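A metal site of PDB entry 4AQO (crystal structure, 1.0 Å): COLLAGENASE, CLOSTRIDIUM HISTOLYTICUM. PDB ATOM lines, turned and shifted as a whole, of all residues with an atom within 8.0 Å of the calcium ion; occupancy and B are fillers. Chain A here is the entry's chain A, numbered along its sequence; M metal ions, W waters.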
ATOM      1  N   ASN A   7      13.305   8.000 -13.183  1.00  0.00           N
ATOM      2  CA  ASN A   7      12.570   8.305 -14.392  1.00  0.00           C
ATOM      3  C   ASN A   7      12.221   7.015 -15.097  1.00  0.00           C
ATOM      4  O   ASN A   7      12.991   6.038 -15.089  1.00  0.00           O
ATOM      5  CB  ASN A   7      13.437   9.124 -15.342  1.00  0.00           C
ATOM      6  CG  ASN A   7      12.695   9.512 -16.613  1.00  0.00           C
ATOM      7  OD1 ASN A   7      11.556   9.997 -16.564  1.00  0.00           O
ATOM      8  ND2 ASN A   7      13.336   9.280 -17.763  1.00  0.00           N
ATOM      9  N   LYS A   8      11.094   7.034 -15.788  1.00  0.00           N
ATOM     10  CA  LYS A   8      10.769   6.012 -16.768  1.00  0.00           C
ATOM     11  C   LYS A   8      10.792   6.631 -18.145  1.00  0.00           C
ATOM     12  O   LYS A   8      10.351   7.780 -18.362  1.00  0.00           O
ATOM     13  CB  LYS A   8       9.451   5.336 -16.468  1.00  0.00           C
ATOM     14  CG  LYS A   8       9.501   4.432 -15.219  1.00  0.00           C
ATOM     15  CD  LYS A   8      10.525   3.295 -15.255  1.00  0.00           C
ATOM     16  CE  LYS A   8      10.272   2.160 -14.260  1.00  0.00           C
ATOM     17  NZ  LYS A   8      10.484   2.661 -12.888  1.00  0.00           N
ATOM     18  N   ALA A   9      11.326   5.882 -19.105  1.00  0.00           N
ATOM     19  CA  ALA A   9      11.357   6.334 -20.484  1.00  0.00           C
ATOM     20  C   ALA A   9       9.930   6.392 -21.051  1.00  0.00           C
ATOM     21  O   ALA A   9       9.047   5.632 -20.614  1.00  0.00           O
ATOM     22  CB  ALA A   9      12.193   5.374 -21.324  1.00  0.00           C
ATOM     23  N   PRO A  10       9.698   7.266 -22.025  1.00  0.00           N
ATOM     24  CA  PRO A  10       8.399   7.377 -22.669  1.00  0.00           C
ATOM     25  C   PRO A  10       8.116   6.193 -23.587  1.00  0.00           C
ATOM     26  O   PRO A  10       9.011   5.368 -23.814  1.00  0.00           O
ATOM     27  CB  PRO A  10       8.550   8.699 -23.472  1.00  0.00           C
ATOM     28  CG  PRO A  10       9.996   8.739 -23.822  1.00  0.00           C
ATOM     29  CD  PRO A  10      10.696   8.190 -22.598  1.00  0.00           C
ATOM     30  N   ILE A  11       6.906   6.137 -24.133  1.00  0.00           N
ATOM     31  CA  ILE A  11       6.498   5.116 -25.105  1.00  0.00           C
ATOM     32  C   ILE A  11       6.003   5.849 -26.348  1.00  0.00           C
ATOM     33  O   ILE A  11       5.099   6.683 -26.276  1.00  0.00           O
ATOM     34  CB  ILE A  11       5.431   4.187 -24.508  1.00  0.00           C
ATOM     35  CG1 ILE A  11       5.998   3.472 -23.270  1.00  0.00           C
ATOM     36  CG2 ILE A  11       4.971   3.188 -25.569  1.00  0.00           C
ATOM     37  CD1 ILE A  11       4.990   2.597 -22.525  1.00  0.00           C
ATOM     38  N   LYS A  34       3.165   8.581 -24.971  1.00  0.00           N
ATOM     39  CA  LYS A  34       2.950   8.849 -23.567  1.00  0.00           C
ATOM     40  C   LYS A  34       4.234   8.801 -22.760  1.00  0.00           C
ATOM     41  O   LYS A  34       5.019   7.872 -22.938  1.00  0.00           O
ATOM     42  CB  LYS A  34       1.996   7.815 -22.955  1.00  0.00           C
ATOM     43  CG  LYS A  34       0.633   7.728 -23.606  1.00  0.00           C
ATOM     44  N   ASP A  35       4.422   9.743 -21.860  1.00  0.00           N
ATOM     45  CA  ASP A  35       5.434   9.624 -20.821  1.00  0.00           C
ATOM     46  C   ASP A  35       4.714   9.565 -19.484  1.00  0.00           C
ATOM     47  O   ASP A  35       4.023  10.486 -19.085  1.00  0.00           O
ATOM     48  CB  ASP A  35       6.422  10.803 -20.843  1.00  0.00           C
ATOM     49  CG  ASP A  35       7.635  10.561 -19.926  1.00  0.00           C
ATOM     50  OD1 ASP A  35       8.044   9.408 -19.761  1.00  0.00           O
ATOM     51  OD2 ASP A  35       8.222  11.514 -19.385  1.00  0.00           O
ATOM     52  N   GLU A  36       4.848   8.448 -18.791  1.00  0.00           N
ATOM     53  CA  GLU A  36       4.041   8.224 -17.591  1.00  0.00           C
ATOM     54  C   GLU A  36       4.369   9.183 -16.454  1.00  0.00           C
ATOM     55  O   GLU A  36       3.537   9.426 -15.599  1.00  0.00           O
ATOM     56  CB  GLU A  36       4.146   6.766 -17.119  1.00  0.00           C
ATOM     57  CG  GLU A  36       5.501   6.370 -16.587  1.00  0.00           C
ATOM     58  CD  GLU A  36       5.588   4.882 -16.436  1.00  0.00           C
ATOM     59  OE1 GLU A  36       5.115   4.352 -15.391  1.00  0.00           O
ATOM     60  OE2 GLU A  36       6.124   4.246 -17.344  1.00  0.00           O
ATOM     61  N   ASP A  37       5.583   9.730 -16.463  1.00  0.00           N
ATOM     62  CA  ASP A  37       6.069  10.509 -15.326  1.00  0.00           C
ATOM     63  C   ASP A  37       6.645  11.849 -15.736  1.00  0.00           C
ATOM     64  O   ASP A  37       7.415  12.430 -14.990  1.00  0.00           O
ATOM     65  CB  ASP A  37       7.070   9.695 -14.500  1.00  0.00           C
ATOM     66  CG  ASP A  37       8.307   9.336 -15.282  1.00  0.00           C
ATOM     67  OD1 ASP A  37       8.389   9.655 -16.487  1.00  0.00           O
ATOM     68  OD2 ASP A  37       9.181   8.710 -14.668  1.00  0.00           O
ATOM     69  N   GLY A  38       6.253  12.345 -16.895  1.00  0.00           N
ATOM     70  CA  GLY A  38       6.815  13.580 -17.406  1.00  0.00           C
ATOM     71  C   GLY A  38       6.192  13.951 -18.728  1.00  0.00           C
ATOM     72  O   GLY A  38       5.032  13.635 -18.982  1.00  0.00           O
ATOM     73  N   LYS A  39       6.970  14.635 -19.551  1.00  0.00           N
ATOM     74  CA  LYS A  39       6.510  15.231 -20.804  1.00  0.00           C
ATOM     75  C   LYS A  39       7.441  14.800 -21.925  1.00  0.00           C
ATOM     76  O   LYS A  39       8.658  14.814 -21.751  1.00  0.00           O
ATOM     77  CB  LYS A  39       6.526  16.806 -20.696  1.00  0.00           C
ATOM     78  CG  LYS A  39       5.904  17.453 -21.904  1.00  0.00           C
ATOM     79  CD  LYS A  39       5.788  18.939 -21.739  1.00  0.00           C
ATOM     80  CE  LYS A  39       5.277  19.583 -23.007  1.00  0.00           C
ATOM     81  NZ  LYS A  39       5.004  21.014 -22.735  1.00  0.00           N
ATOM     82  N   ILE A  40       6.876  14.544 -23.092  1.00  0.00           N
ATOM     83  CA  ILE A  40       7.678  14.373 -24.308  1.00  0.00           C
ATOM     84  C   ILE A  40       7.999  15.741 -24.874  1.00  0.00           C
ATOM     85  O   ILE A  40       7.098  16.557 -25.121  1.00  0.00           O
ATOM     86  CB  ILE A  40       6.965  13.476 -25.324  1.00  0.00           C
ATOM     87  CG1 ILE A  40       6.866  12.046 -24.750  1.00  0.00           C
ATOM     88  CG2 ILE A  40       7.692  13.508 -26.664  1.00  0.00           C
ATOM     89  CD1 ILE A  40       5.955  11.127 -25.550  1.00  0.00           C
ATOM     90  N   THR A  75      11.558  11.746 -27.059  1.00  0.00           N
ATOM     91  CA  THR A  75      12.483  12.041 -25.984  1.00  0.00           C
ATOM     92  C   THR A  75      11.703  12.746 -24.876  1.00  0.00           C
ATOM     93  O   THR A  75      10.942  13.696 -25.171  1.00  0.00           O
ATOM     94  CB  THR A  75      13.621  12.965 -26.468  1.00  0.00           C
ATOM     95  OG1 THR A  75      14.285  12.326 -27.568  1.00  0.00           O
ATOM     96  CG2 THR A  75      14.667  13.186 -25.370  1.00  0.00           C
ATOM     97  N   ASP A  76      11.868  12.287 -23.628  1.00  0.00           N
ATOM     98  CA  ASP A  76      11.192  12.937 -22.512  1.00  0.00           C
ATOM     99  C   ASP A  76      12.028  14.074 -21.931  1.00  0.00           C
ATOM    100  O   ASP A  76      13.118  14.378 -22.404  1.00  0.00           O
ATOM    101  CB  ASP A  76      10.709  11.920 -21.439  1.00  0.00           C
ATOM    102  CG  ASP A  76      11.825  11.314 -20.580  1.00  0.00           C
ATOM    103  OD1 ASP A  76      12.967  11.811 -20.639  1.00  0.00           O
ATOM    104  OD2 ASP A  76      11.491  10.333 -19.854  1.00  0.00           O
ATOM    105  N   ASP A  77      11.465  14.701 -20.908  1.00  0.00           N
ATOM    106  CA  ASP A  77      12.053  15.884 -20.316  1.00  0.00           C
ATOM    107  C   ASP A  77      13.345  15.607 -19.531  1.00  0.00           C
ATOM    108  O   ASP A  77      14.050  16.544 -19.157  1.00  0.00           O
ATOM    109  CB  ASP A  77      11.023  16.615 -19.417  1.00  0.00           C
ATOM    110  CG  ASP A  77      10.550  15.721 -18.285  1.00  0.00           C
ATOM    111  OD1 ASP A  77       9.792  14.757 -18.588  1.00  0.00           O
ATOM    112  OD2 ASP A  77      10.955  15.958 -17.125  1.00  0.00           O
ATOM    113  N   LYS A  78      13.664  14.317 -19.313  1.00  0.00           N
ATOM    114  CA  LYS A  78      14.934  13.910 -18.721  1.00  0.00           C
ATOM    115  C   LYS A  78      15.952  13.472 -19.755  1.00  0.00           C
ATOM    116  O   LYS A  78      17.125  13.220 -19.405  1.00  0.00           O
ATOM    117  CB  LYS A  78      14.709  12.787 -17.703  1.00  0.00           C
ATOM    118  CG  LYS A  78      13.798  13.177 -16.558  1.00  0.00           C
ATOM    119  CD  LYS A  78      14.507  14.153 -15.625  1.00  0.00           C
ATOM    120  N   GLY A  79      15.556  13.383 -21.014  1.00  0.00           N
ATOM    121  CA  GLY A  79      16.433  12.903 -22.062  1.00  0.00           C
ATOM    122  C   GLY A  79      16.347  11.429 -22.380  1.00  0.00           C
ATOM    123  O   GLY A  79      17.136  10.938 -23.197  1.00  0.00           O
ATOM    124  N   ALA A  80      15.423  10.681 -21.760  1.00  0.00           N
ATOM    125  CA  ALA A  80      15.240   9.293 -22.087  1.00  0.00           C
ATOM    126  C   ALA A  80      14.447   9.172 -23.379  1.00  0.00           C
ATOM    127  O   ALA A  80      13.558   9.973 -23.672  1.00  0.00           O
ATOM    128  CB  ALA A  80      14.498   8.579 -20.959  1.00  0.00           C
ATOM    129  N   THR A  81      14.761   8.136 -24.176  1.00  0.00           N
ATOM    130  CA  THR A  81      14.204   7.983 -25.506  1.00  0.00           C
ATOM    131  C   THR A  81      13.527   6.637 -25.706  1.00  0.00           C
ATOM    132  O   THR A  81      13.826   5.644 -25.039  1.00  0.00           O
ATOM    133  CB  THR A  81      15.302   8.175 -26.583  1.00  0.00           C
ATOM    134  OG1 THR A  81      16.255   7.105 -26.479  1.00  0.00           O
ATOM    135  CG2 THR A  81      15.994   9.510 -26.462  1.00  0.00           C
HETATM  136 CA    CA M   1       9.802  10.074 -18.235  1.00  0.00          CA
HETATM  137  O   HOH W   1      10.310  12.337 -17.498  1.00  0.00           O
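The backbone NH (N) of Gly 79 is in hydrogen-bond range of the side-chain carboxylate (OD1) of Asp 76 (3.1 Å). The backbone NH of Lys 78 is in hydrogen-bond range of the side-chain carboxylate of Asp 76, 2.9 Å away. The side-chain carboxylate of Asp 35 sits close to the backbone NH of Lys 39. OD2 of Asp 35 lies close to N of Gly 38, at 3.3 Å. OD1 of Asp 76 lies within hydrogen-bond range of N of Ala 80 (2.9 Å).
The calcium ion is bound by OD1 of Asp 37 (2.3 Å), OD2 of Asp 76 (2.4 Å), O of Lys 8 (2.4 Å), OD1 of Asp 35 (2.4 Å), OD1 of Asn 7 (2.4 Å), OD2 of Asp 35 (2.4 Å) and water W1 (2.4 Å).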
